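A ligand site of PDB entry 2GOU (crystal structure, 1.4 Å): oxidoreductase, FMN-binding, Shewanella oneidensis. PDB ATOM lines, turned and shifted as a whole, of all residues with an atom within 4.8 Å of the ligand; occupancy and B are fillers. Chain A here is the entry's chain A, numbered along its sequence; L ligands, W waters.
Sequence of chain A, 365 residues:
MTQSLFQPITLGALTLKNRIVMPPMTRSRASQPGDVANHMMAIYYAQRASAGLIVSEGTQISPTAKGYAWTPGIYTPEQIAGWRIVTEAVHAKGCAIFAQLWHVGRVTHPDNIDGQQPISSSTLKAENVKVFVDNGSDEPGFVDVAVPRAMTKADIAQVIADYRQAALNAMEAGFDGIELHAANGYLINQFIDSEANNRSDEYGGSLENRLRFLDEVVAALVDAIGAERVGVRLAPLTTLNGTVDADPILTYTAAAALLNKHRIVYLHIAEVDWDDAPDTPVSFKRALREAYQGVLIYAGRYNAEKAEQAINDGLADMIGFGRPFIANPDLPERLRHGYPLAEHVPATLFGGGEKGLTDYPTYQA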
ATOM      1  N   PRO A  23     -16.845  -4.124 -14.560  1.00  0.00           N
ATOM      2  CA  PRO A  23     -16.011  -3.652 -13.454  1.00  0.00           C
ATOM      3  C   PRO A  23     -16.059  -2.143 -13.320  1.00  0.00           C
ATOM      4  O   PRO A  23     -16.447  -1.452 -14.242  1.00  0.00           O
ATOM      5  CB  PRO A  23     -14.628  -4.169 -13.830  1.00  0.00           C
ATOM      6  CG  PRO A  23     -14.621  -4.004 -15.321  1.00  0.00           C
ATOM      7  CD  PRO A  23     -16.028  -4.431 -15.748  1.00  0.00           C
ATOM      8  N   PRO A  24     -15.672  -1.628 -12.149  1.00  0.00           N
ATOM      9  CA  PRO A  24     -15.683  -0.193 -11.892  1.00  0.00           C
ATOM     10  C   PRO A  24     -14.774   0.557 -12.850  1.00  0.00           C
ATOM     11  O   PRO A  24     -13.590   0.233 -12.974  1.00  0.00           O
ATOM     12  CB  PRO A  24     -15.198  -0.099 -10.438  1.00  0.00           C
ATOM     13  CG  PRO A  24     -14.305  -1.294 -10.298  1.00  0.00           C
ATOM     14  CD  PRO A  24     -15.065  -2.370 -11.033  1.00  0.00           C
ATOM     15  N   MET A  25     -15.323   1.566 -13.534  1.00  0.00           N
ATOM     16  CA  MET A  25     -14.502   2.332 -14.462  1.00  0.00           C
ATOM     17  C   MET A  25     -14.809   3.818 -14.443  1.00  0.00           C
ATOM     18  O   MET A  25     -15.858   4.282 -14.906  1.00  0.00           O
ATOM     19  CB  MET A  25     -14.636   1.811 -15.889  1.00  0.00           C
ATOM     20  CG  MET A  25     -14.036   0.429 -16.069  1.00  0.00           C
ATOM     21  SD  MET A  25     -14.180  -0.187 -17.765  1.00  0.00           S
ATOM     22  CE  MET A  25     -15.955  -0.499 -17.858  1.00  0.00           C
ATOM     23  N   THR A  26     -13.861   4.564 -13.888  1.00  0.00           N
ATOM     24  CA  THR A  26     -13.923   6.019 -13.827  1.00  0.00           C
ATOM     25  C   THR A  26     -14.059   6.589 -15.231  1.00  0.00           C
ATOM     26  O   THR A  26     -13.274   6.255 -16.114  1.00  0.00           O
ATOM     27  CB  THR A  26     -12.612   6.548 -13.197  1.00  0.00           C
ATOM     28  OG1 THR A  26     -12.585   6.191 -11.818  1.00  0.00           O
ATOM     29  CG2 THR A  26     -12.499   8.059 -13.332  1.00  0.00           C
ATOM     30  N   ARG A  27     -15.073   7.428 -15.439  1.00  0.00           N
ATOM     31  CA  ARG A  27     -15.275   8.073 -16.745  1.00  0.00           C
ATOM     32  C   ARG A  27     -15.242   9.599 -16.611  1.00  0.00           C
ATOM     33  O   ARG A  27     -15.239  10.316 -17.614  1.00  0.00           O
ATOM     34  CB  ARG A  27     -16.596   7.634 -17.374  1.00  0.00           C
ATOM     35  CG  ARG A  27     -16.747   6.113 -17.547  1.00  0.00           C
ATOM     36  CD  ARG A  27     -15.583   5.470 -18.300  1.00  0.00           C
ATOM     37  NE  ARG A  27     -15.381   6.083 -19.613  1.00  0.00           N
ATOM     38  CZ  ARG A  27     -16.089   5.777 -20.690  1.00  0.00           C
ATOM     39  NH1 ARG A  27     -17.034   4.846 -20.659  1.00  0.00           N
ATOM     40  NH2 ARG A  27     -15.888   6.456 -21.820  1.00  0.00           N
ATOM     41  N   GLU A  57     -18.259   3.138 -11.253  1.00  0.00           N
ATOM     42  CA  GLU A  57     -16.957   3.775 -11.248  1.00  0.00           C
ATOM     43  C   GLU A  57     -16.722   4.189  -9.793  1.00  0.00           C
ATOM     44  O   GLU A  57     -17.672   4.391  -9.018  1.00  0.00           O
ATOM     45  CB  GLU A  57     -17.020   5.043 -12.105  1.00  0.00           C
ATOM     46  CG  GLU A  57     -18.119   5.996 -11.650  1.00  0.00           C
ATOM     47  CD  GLU A  57     -18.646   6.862 -12.777  1.00  0.00           C
ATOM     48  OE1 GLU A  57     -18.148   7.986 -12.970  1.00  0.00           O
ATOM     49  OE2 GLU A  57     -19.580   6.420 -13.482  1.00  0.00           O
ATOM     50  N   GLY A  58     -15.457   4.357  -9.423  1.00  0.00           N
ATOM     51  CA  GLY A  58     -15.149   4.797  -8.074  1.00  0.00           C
ATOM     52  C   GLY A  58     -15.908   6.073  -7.755  1.00  0.00           C
ATOM     53  O   GLY A  58     -15.986   6.997  -8.566  1.00  0.00           O
ATOM     54  N   GLN A 100     -18.919   1.551  -6.011  1.00  0.00           N
ATOM     55  CA  GLN A 100     -17.551   1.362  -5.540  1.00  0.00           C
ATOM     56  C   GLN A 100     -17.142   2.566  -4.699  1.00  0.00           C
ATOM     57  O   GLN A 100     -16.911   3.654  -5.215  1.00  0.00           O
ATOM     58  CB  GLN A 100     -16.551   1.204  -6.689  1.00  0.00           C
ATOM     59  CG  GLN A 100     -15.177   0.844  -6.131  1.00  0.00           C
ATOM     60  CD  GLN A 100     -14.052   0.833  -7.150  1.00  0.00           C
ATOM     61  OE1 GLN A 100     -13.779   1.841  -7.792  1.00  0.00           O
ATOM     62  NE2 GLN A 100     -13.385  -0.313  -7.271  1.00  0.00           N
ATOM     63  N   TRP A 102     -14.842   4.919  -2.805  1.00  0.00           N
ATOM     64  CA  TRP A 102     -13.465   5.292  -3.052  1.00  0.00           C
ATOM     65  C   TRP A 102     -12.809   6.323  -2.151  1.00  0.00           C
ATOM     66  O   TRP A 102     -13.408   7.344  -1.817  1.00  0.00           O
ATOM     67  CB  TRP A 102     -13.414   5.825  -4.480  1.00  0.00           C
ATOM     68  CG  TRP A 102     -12.128   5.752  -5.231  1.00  0.00           C
ATOM     69  CD1 TRP A 102     -11.000   5.028  -4.909  1.00  0.00           C
ATOM     70  CD2 TRP A 102     -11.894   6.283  -6.541  1.00  0.00           C
ATOM     71  NE1 TRP A 102     -10.106   5.075  -5.965  1.00  0.00           N
ATOM     72  CE2 TRP A 102     -10.637   5.828  -6.974  1.00  0.00           C
ATOM     73  CE3 TRP A 102     -12.661   7.088  -7.401  1.00  0.00           C
ATOM     74  CZ2 TRP A 102     -10.110   6.155  -8.227  1.00  0.00           C
ATOM     75  CZ3 TRP A 102     -12.142   7.410  -8.651  1.00  0.00           C
ATOM     76  CH2 TRP A 102     -10.884   6.939  -9.052  1.00  0.00           C
ATOM     77  N   HIS A 181     -13.166  -0.165  -2.582  1.00  0.00           N
ATOM     78  CA  HIS A 181     -11.973  -0.124  -3.434  1.00  0.00           C
ATOM     79  C   HIS A 181     -10.744  -0.176  -2.521  1.00  0.00           C
ATOM     80  O   HIS A 181     -10.325   0.846  -1.974  1.00  0.00           O
ATOM     81  CB  HIS A 181     -11.926   1.155  -4.269  1.00  0.00           C
ATOM     82  CG  HIS A 181     -10.970   1.085  -5.411  1.00  0.00           C
ATOM     83  ND1 HIS A 181     -10.007   0.098  -5.517  1.00  0.00           N
ATOM     84  CD2 HIS A 181     -10.830   1.876  -6.510  1.00  0.00           C
ATOM     85  CE1 HIS A 181      -9.324   0.280  -6.641  1.00  0.00           C
ATOM     86  NE2 HIS A 181      -9.807   1.347  -7.252  1.00  0.00           N
ATOM     87  N   ASN A 184      -5.696  -1.159  -6.508  1.00  0.00           N
ATOM     88  CA  ASN A 184      -5.005  -0.227  -7.387  1.00  0.00           C
ATOM     89  C   ASN A 184      -4.279   0.953  -6.780  1.00  0.00           C
ATOM     90  O   ASN A 184      -4.322   2.075  -7.290  1.00  0.00           O
ATOM     91  CB  ASN A 184      -5.978   0.205  -8.496  1.00  0.00           C
ATOM     92  CG  ASN A 184      -6.542  -1.001  -9.230  1.00  0.00           C
ATOM     93  OD1 ASN A 184      -5.998  -2.095  -9.140  1.00  0.00           O
ATOM     94  ND2 ASN A 184      -7.633  -0.803  -9.969  1.00  0.00           N
ATOM     95  N   ARG A 233     -12.540  -5.057  -3.329  1.00  0.00           N
ATOM     96  CA  ARG A 233     -11.619  -5.230  -4.446  1.00  0.00           C
ATOM     97  C   ARG A 233     -10.177  -5.110  -3.956  1.00  0.00           C
ATOM     98  O   ARG A 233      -9.848  -4.205  -3.206  1.00  0.00           O
ATOM     99  CB  ARG A 233     -11.863  -4.170  -5.539  1.00  0.00           C
ATOM    100  CG  ARG A 233     -11.226  -4.579  -6.872  1.00  0.00           C
ATOM    101  CD  ARG A 233     -11.597  -3.669  -8.025  1.00  0.00           C
ATOM    102  NE  ARG A 233     -11.627  -4.446  -9.269  1.00  0.00           N
ATOM    103  CZ  ARG A 233     -11.370  -3.971 -10.485  1.00  0.00           C
ATOM    104  NH1 ARG A 233     -11.043  -2.699 -10.657  1.00  0.00           N
ATOM    105  NH2 ARG A 233     -11.490  -4.771 -11.530  1.00  0.00           N
ATOM    106  N   ALA A 270      -8.428  -7.382  -9.023  1.00  0.00           N
ATOM    107  CA  ALA A 270      -8.045  -6.562 -10.178  1.00  0.00           C
ATOM    108  C   ALA A 270      -6.708  -7.159 -10.620  1.00  0.00           C
ATOM    109  O   ALA A 270      -5.647  -6.808 -10.093  1.00  0.00           O
ATOM    110  CB  ALA A 270      -7.889  -5.118  -9.772  1.00  0.00           C
ATOM    111  N   VAL A 272      -5.258  -7.058 -13.703  1.00  0.00           N
ATOM    112  CA  VAL A 272      -4.489  -6.217 -14.604  1.00  0.00           C
ATOM    113  C   VAL A 272      -4.955  -4.793 -14.367  1.00  0.00           C
ATOM    114  O   VAL A 272      -6.135  -4.560 -14.082  1.00  0.00           O
ATOM    115  CB  VAL A 272      -4.766  -6.544 -16.097  1.00  0.00           C
ATOM    116  CG1 VAL A 272      -4.041  -5.548 -17.003  1.00  0.00           C
ATOM    117  CG2 VAL A 272      -4.345  -7.969 -16.418  1.00  0.00           C
ATOM    118  N   ASP A 273      -4.032  -3.850 -14.423  1.00  0.00           N
ATOM    119  CA  ASP A 273      -4.391  -2.437 -14.324  1.00  0.00           C
ATOM    120  C   ASP A 273      -3.702  -1.805 -15.524  1.00  0.00           C
ATOM    121  O   ASP A 273      -2.468  -1.722 -15.572  1.00  0.00           O
ATOM    122  CB  ASP A 273      -3.908  -1.788 -13.022  1.00  0.00           C
ATOM    123  CG  ASP A 273      -4.717  -0.544 -12.667  1.00  0.00           C
ATOM    124  OD1 ASP A 273      -4.154   0.355 -12.011  1.00  0.00           O
ATOM    125  OD2 ASP A 273      -5.912  -0.469 -13.038  1.00  0.00           O
ATOM    126  N   TRP A 274      -4.498  -1.388 -16.496  1.00  0.00           N
ATOM    127  CA  TRP A 274      -4.006  -0.797 -17.744  1.00  0.00           C
ATOM    128  C   TRP A 274      -3.064  -1.784 -18.439  1.00  0.00           C
ATOM    129  O   TRP A 274      -3.527  -2.800 -18.936  1.00  0.00           O
ATOM    130  CB  TRP A 274      -3.358   0.565 -17.470  1.00  0.00           C
ATOM    131  CG  TRP A 274      -4.374   1.521 -16.906  1.00  0.00           C
ATOM    132  CD1 TRP A 274      -4.567   1.835 -15.588  1.00  0.00           C
ATOM    133  CD2 TRP A 274      -5.416   2.203 -17.620  1.00  0.00           C
ATOM    134  NE1 TRP A 274      -5.650   2.659 -15.446  1.00  0.00           N
ATOM    135  CE2 TRP A 274      -6.197   2.895 -16.685  1.00  0.00           C
ATOM    136  CE3 TRP A 274      -5.755   2.270 -18.990  1.00  0.00           C
ATOM    137  CZ2 TRP A 274      -7.307   3.674 -17.050  1.00  0.00           C
ATOM    138  CZ3 TRP A 274      -6.857   3.046 -19.344  1.00  0.00           C
ATOM    139  CH2 TRP A 274      -7.622   3.733 -18.385  1.00  0.00           C
ATOM    140  N   ALA A 299     -10.885  -9.570 -12.916  1.00  0.00           N
ATOM    141  CA  ALA A 299     -10.976  -8.701 -14.072  1.00  0.00           C
ATOM    142  C   ALA A 299      -9.557  -8.358 -14.505  1.00  0.00           C
ATOM    143  O   ALA A 299      -8.677  -8.183 -13.674  1.00  0.00           O
ATOM    144  CB  ALA A 299     -11.755  -7.424 -13.739  1.00  0.00           C
ATOM    145  N   GLY A 300      -9.365  -8.279 -15.811  1.00  0.00           N
ATOM    146  CA  GLY A 300      -8.048  -7.938 -16.339  1.00  0.00           C
ATOM    147  C   GLY A 300      -7.692  -8.721 -17.588  1.00  0.00           C
ATOM    148  O   GLY A 300      -7.286  -9.883 -17.496  1.00  0.00           O
ATOM    149  N   ARG A 301      -7.859  -8.088 -18.746  1.00  0.00           N
ATOM    150  CA  ARG A 301      -7.536  -8.679 -20.032  1.00  0.00           C
ATOM    151  C   ARG A 301      -8.204 -10.011 -20.330  1.00  0.00           C
ATOM    152  O   ARG A 301      -7.630 -10.875 -21.004  1.00  0.00           O
ATOM    153  CB  ARG A 301      -6.022  -8.819 -20.195  1.00  0.00           C
ATOM    154  CG  ARG A 301      -5.274  -7.498 -20.236  1.00  0.00           C
ATOM    155  CD  ARG A 301      -5.739  -6.606 -21.364  1.00  0.00           C
ATOM    156  NE  ARG A 301      -4.804  -5.508 -21.595  1.00  0.00           N
ATOM    157  CZ  ARG A 301      -5.073  -4.426 -22.307  1.00  0.00           C
ATOM    158  NH1 ARG A 301      -6.268  -4.269 -22.870  1.00  0.00           N
ATOM    159  NH2 ARG A 301      -4.148  -3.493 -22.473  1.00  0.00           N
ATOM    160  N   TYR A 302      -9.409 -10.207 -19.828  1.00  0.00           N
ATOM    161  CA  TYR A 302     -10.108 -11.446 -20.135  1.00  0.00           C
ATOM    162  C   TYR A 302     -10.843 -11.324 -21.453  1.00  0.00           C
ATOM    163  O   TYR A 302     -11.262 -10.247 -21.853  1.00  0.00           O
ATOM    164  CB  TYR A 302     -11.131 -11.777 -19.046  1.00  0.00           C
ATOM    165  CG  TYR A 302     -10.518 -12.429 -17.851  1.00  0.00           C
ATOM    166  CD1 TYR A 302     -10.370 -13.819 -17.790  1.00  0.00           C
ATOM    167  CD2 TYR A 302     -10.015 -11.664 -16.808  1.00  0.00           C
ATOM    168  CE1 TYR A 302      -9.734 -14.424 -16.715  1.00  0.00           C
ATOM    169  CE2 TYR A 302      -9.362 -12.255 -15.732  1.00  0.00           C
ATOM    170  CZ  TYR A 302      -9.228 -13.634 -15.685  1.00  0.00           C
ATOM    171  OH  TYR A 302      -8.544 -14.217 -14.665  1.00  0.00           O
ATOM    172  N   GLY A 320     -14.968  -9.961 -14.867  1.00  0.00           N
ATOM    173  CA  GLY A 320     -15.245  -8.617 -15.305  1.00  0.00           C
ATOM    174  C   GLY A 320     -14.494  -8.309 -16.586  1.00  0.00           C
ATOM    175  O   GLY A 320     -13.370  -8.789 -16.801  1.00  0.00           O
ATOM    176  N   PHE A 321     -15.137  -7.534 -17.452  1.00  0.00           N
ATOM    177  CA  PHE A 321     -14.552  -7.090 -18.718  1.00  0.00           C
ATOM    178  C   PHE A 321     -14.697  -5.591 -18.678  1.00  0.00           C
ATOM    179  O   PHE A 321     -15.808  -5.052 -18.712  1.00  0.00           O
ATOM    180  CB  PHE A 321     -15.361  -7.639 -19.903  1.00  0.00           C
ATOM    181  CG  PHE A 321     -15.398  -9.131 -19.973  1.00  0.00           C
ATOM    182  CD1 PHE A 321     -14.514  -9.816 -20.805  1.00  0.00           C
ATOM    183  CD2 PHE A 321     -16.324  -9.851 -19.234  1.00  0.00           C
ATOM    184  CE1 PHE A 321     -14.566 -11.203 -20.893  1.00  0.00           C
ATOM    185  CE2 PHE A 321     -16.384 -11.244 -19.318  1.00  0.00           C
ATOM    186  CZ  PHE A 321     -15.497 -11.912 -20.147  1.00  0.00           C
ATOM    187  N   GLY A 322     -13.559  -4.904 -18.592  1.00  0.00           N
ATOM    188  CA  GLY A 322     -13.576  -3.461 -18.486  1.00  0.00           C
ATOM    189  C   GLY A 322     -13.580  -2.727 -19.804  1.00  0.00           C
ATOM    190  O   GLY A 322     -14.628  -2.297 -20.284  1.00  0.00           O
ATOM    191  N   ARG A 323     -12.407  -2.597 -20.403  1.00  0.00           N
ATOM    192  CA  ARG A 323     -12.323  -1.889 -21.665  1.00  0.00           C
ATOM    193  C   ARG A 323     -13.309  -2.397 -22.727  1.00  0.00           C
ATOM    194  O   ARG A 323     -13.906  -1.599 -23.452  1.00  0.00           O
ATOM    195  CB  ARG A 323     -10.861  -1.891 -22.119  1.00  0.00           C
ATOM    196  CG  ARG A 323     -10.072  -0.850 -21.325  1.00  0.00           C
ATOM    197  CD  ARG A 323      -8.566  -1.054 -21.338  1.00  0.00           C
ATOM    198  NE  ARG A 323      -8.150  -2.159 -20.479  1.00  0.00           N
ATOM    199  CZ  ARG A 323      -6.883  -2.397 -20.160  1.00  0.00           C
ATOM    200  NH1 ARG A 323      -6.573  -3.434 -19.387  1.00  0.00           N
ATOM    201  NH2 ARG A 323      -5.920  -1.610 -20.621  1.00  0.00           N
ATOM    202  N   PRO A 324     -13.511  -3.725 -22.820  1.00  0.00           N
ATOM    203  CA  PRO A 324     -14.482  -4.171 -23.825  1.00  0.00           C
ATOM    204  C   PRO A 324     -15.903  -3.654 -23.545  1.00  0.00           C
ATOM    205  O   PRO A 324     -16.673  -3.434 -24.475  1.00  0.00           O
ATOM    206  CB  PRO A 324     -14.406  -5.695 -23.727  1.00  0.00           C
ATOM    207  CG  PRO A 324     -12.956  -5.916 -23.391  1.00  0.00           C
ATOM    208  CD  PRO A 324     -12.704  -4.855 -22.334  1.00  0.00           C
ATOM    209  N   ILE A 326     -16.653  -0.779 -22.271  1.00  0.00           N
ATOM    210  CA  ILE A 326     -16.720   0.629 -22.629  1.00  0.00           C
ATOM    211  C   ILE A 326     -17.214   0.765 -24.076  1.00  0.00           C
ATOM    212  O   ILE A 326     -18.121   1.549 -24.354  1.00  0.00           O
ATOM    213  CB  ILE A 326     -15.331   1.298 -22.519  1.00  0.00           C
ATOM    214  CG1 ILE A 326     -14.931   1.338 -21.045  1.00  0.00           C
ATOM    215  CG2 ILE A 326     -15.337   2.679 -23.171  1.00  0.00           C
ATOM    216  CD1 ILE A 326     -13.611   2.021 -20.771  1.00  0.00           C
ATOM    217  N   LEU A 349     -12.090   8.433 -22.792  1.00  0.00           N
ATOM    218  CA  LEU A 349     -12.321   7.677 -21.571  1.00  0.00           C
ATOM    219  C   LEU A 349     -12.689   8.596 -20.414  1.00  0.00           C
ATOM    220  O   LEU A 349     -13.576   8.268 -19.612  1.00  0.00           O
ATOM    221  CB  LEU A 349     -11.068   6.880 -21.186  1.00  0.00           C
ATOM    222  CG  LEU A 349     -10.749   5.674 -22.060  1.00  0.00           C
ATOM    223  CD1 LEU A 349      -9.399   5.095 -21.657  1.00  0.00           C
ATOM    224  CD2 LEU A 349     -11.858   4.633 -21.932  1.00  0.00           C
ATOM    225  N   PHE A 350     -12.032   9.744 -20.326  1.00  0.00           N
ATOM    226  CA  PHE A 350     -12.238  10.680 -19.217  1.00  0.00           C
ATOM    227  C   PHE A 350     -12.672  12.069 -19.640  1.00  0.00           C
ATOM    228  O   PHE A 350     -12.096  12.665 -20.551  1.00  0.00           O
ATOM    229  CB  PHE A 350     -10.950  10.808 -18.408  1.00  0.00           C
ATOM    230  CG  PHE A 350     -10.338   9.492 -18.031  1.00  0.00           C
ATOM    231  CD1 PHE A 350      -9.168   9.047 -18.637  1.00  0.00           C
ATOM    232  CD2 PHE A 350     -10.956   8.676 -17.088  1.00  0.00           C
ATOM    233  CE1 PHE A 350      -8.619   7.823 -18.308  1.00  0.00           C
ATOM    234  CE2 PHE A 350     -10.408   7.439 -16.753  1.00  0.00           C
ATOM    235  CZ  PHE A 350      -9.237   7.007 -17.366  1.00  0.00           C
HETATM  236  N1  LIG L   1     -10.748   0.089 -11.352  1.00  0.00           N
HETATM  237  C1  LIG L   1     -11.385   0.376 -10.127  1.00  0.00           C
HETATM  238  O1  LIG L   1     -11.325  -0.353  -9.198  1.00  0.00           O
HETATM  239  N2  LIG L   1     -12.065   1.636 -10.007  1.00  0.00           N
HETATM  240  C2  LIG L   1     -12.172   2.572 -10.980  1.00  0.00           C
HETATM  241  O2  LIG L   1     -12.891   3.719 -10.806  1.00  0.00           O
HETATM  242  C3  LIG L   1     -11.388   2.324 -12.227  1.00  0.00           C
HETATM  243  N3  LIG L   1     -11.465   3.210 -13.259  1.00  0.00           N
HETATM  244  C4  LIG L   1     -11.062   2.794 -14.491  1.00  0.00           C
HETATM  245  C5  LIG L   1     -11.288   3.678 -15.655  1.00  0.00           C
HETATM  246  C6  LIG L   1     -11.015   3.231 -16.997  1.00  0.00           C
HETATM  247  C7  LIG L   1     -11.514   4.135 -18.125  1.00  0.00           C
HETATM  248  C8  LIG L   1     -10.581   1.889 -17.238  1.00  0.00           C
HETATM  249  C9  LIG L   1     -10.217   1.237 -18.602  1.00  0.00           C
HETATM  250  C10 LIG L   1     -10.141   1.061 -16.173  1.00  0.00           C
HETATM  251  C11 LIG L   1     -10.482   1.479 -14.747  1.00  0.00           C
HETATM  252  N4  LIG L   1     -10.414   0.610 -13.610  1.00  0.00           N
HETATM  253  C12 LIG L   1     -10.809   0.962 -12.345  1.00  0.00           C
HETATM  254  C13 LIG L   1      -9.844  -0.771 -13.796  1.00  0.00           C
HETATM  255  C14 LIG L   1     -10.927  -1.729 -14.332  1.00  0.00           C
HETATM  256  O3  LIG L   1     -11.987  -1.953 -13.395  1.00  0.00           O
HETATM  257  C15 LIG L   1     -10.370  -3.093 -14.742  1.00  0.00           C
HETATM  258  O4  LIG L   1      -9.888  -3.791 -13.580  1.00  0.00           O
HETATM  259  C16 LIG L   1      -9.232  -2.985 -15.734  1.00  0.00           C
HETATM  260  O5  LIG L   1      -9.571  -2.118 -16.858  1.00  0.00           O
HETATM  261  C17 LIG L   1      -8.768  -4.333 -16.250  1.00  0.00           C
HETATM  262  O6  LIG L   1      -9.826  -5.015 -17.003  1.00  0.00           O
HETATM  263  P1  LIG L   1      -9.875  -4.977 -18.589  1.00  0.00           P
HETATM  264  O7  LIG L   1     -10.211  -3.589 -19.028  1.00  0.00           O
HETATM  265  O8  LIG L   1      -8.519  -5.459 -19.070  1.00  0.00           O
HETATM  266  O9  LIG L   1     -10.994  -5.964 -18.932  1.00  0.00           O
HETATM  267  O   HOH W   1      -7.222  -0.616 -17.005  1.00  0.00           O
HETATM  268  O   HOH W   2      -8.771   2.186 -10.046  1.00  0.00           O
HETATM  269  O   HOH W   3      -8.729  -5.597 -22.134  1.00  0.00           O
HETATM  270  O   HOH W   4     -11.046  -8.475 -18.069  1.00  0.00           O
HETATM  271  O   HOH W   5      -7.574   1.697 -12.379  1.00  0.00           O
HETATM  272  O   HOH W   6      -7.565  -2.751 -12.581  1.00  0.00           O
HETATM  273  O   HOH W   7     -10.751  -7.437 -21.319  1.00  0.00           O
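Water W6 lies within hydrogen-bond range of an oxygen (O4) of the ligand (2.7 Å), the backbone carbonyl oxygen of Val 272 (2.8 Å), the side-chain carboxylate of Asp 273 (2.9 Å) and the side-chain amide nitrogen of Asn 184 (3.3 Å).
Water W1 bridges O5 of the ligand and N of Trp 274.
Water W7 bridges an oxygen (O9) of the ligand (2.8 Å) and the backbone carbonyl oxygen (O) of Tyr 302 (2.9 Å).
Water W3 lies within hydrogen-bond range of NH1 of Arg 301 and O8 of the ligand.
Water W2 lies within hydrogen-bond range of a ring nitrogen (NE2) of His 181 (3.1 Å), a nitrogen (N1) of the ligand (3.2 Å) and the side-chain amide nitrogen of Asn 184 (3.2 Å).
Water W5 lies within hydrogen-bond range of the side-chain carboxylate (OD2) of Asp 273 (2.8 Å) and the side-chain amide nitrogen (ND2) of Asn 184 (3.5 Å).
The side-chain amide oxygen (OE1) of Gln 100 sits close to the backbone NH (N) of Gly 58.
The backbone carbonyl oxygen of Trp 274 is in hydrogen-bond range of the guanidinium group of Arg 323 (3.1 Å).
The backbone carbonyl oxygen of Leu 349 is in hydrogen-bond range of the guanidinium group of Arg 27 (2.8 Å).
NH1 of Arg 233 lies within hydrogen-bond range of O1 of the ligand (2.8 Å).
The backbone NH (N) of Arg 301 lies within hydrogen-bond range of an oxygen (O8) of the ligand (2.7 Å).
The guanidinium group of Arg 323 is in salt-bridge range of an oxygen (O8) of the ligand (2.8 Å).
O2 of the ligand sits at hydrogen-bond distance from OG1 of Thr 26 (2.7 Å).
N of Arg 323 is in hydrogen-bond range of O7 of the ligand, 2.8 Å away.
An oxygen (O9) of the ligand is in hydrogen-bond range of the backbone NH (N) of Gly 322.
The backbone carbonyl oxygen (O) of Pro 24 is in hydrogen-bond range of an oxygen (O3) of the ligand (2.7 Å).
NE2 of His 181 is in hydrogen-bond range of O1 of the ligand.
N3 of the ligand lies within hydrogen-bond range of N of Thr 26, 2.8 Å away.
OE1 of Gln 100 sits at hydrogen-bond distance from N2 of the ligand (2.8 Å).
The backbone NH of Gly 58 is in hydrogen-bond range of an oxygen (O2) of the ligand, at 3.0 Å.
Residues that only touch the ligand: Met 25 (3.4 Å), Val 272 (3.4 Å), Pro 23 (3.5 Å), Gly 300 (3.5 Å), Asn 184 (3.5 Å), Trp 274 (3.6 Å), Phe 321 (3.7 Å), Phe 350 (3.7 Å), Leu 349 (3.9 Å), Pro 324 (3.97 Å), Ile 326 (3.98 Å) and Glu 57 (3.99 Å).
Of the 28 residues printed, 21 come within 4 Å of the ligand.
The nearest printed residue that does not touch the ligand is Asp 273 (4.02 Å).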
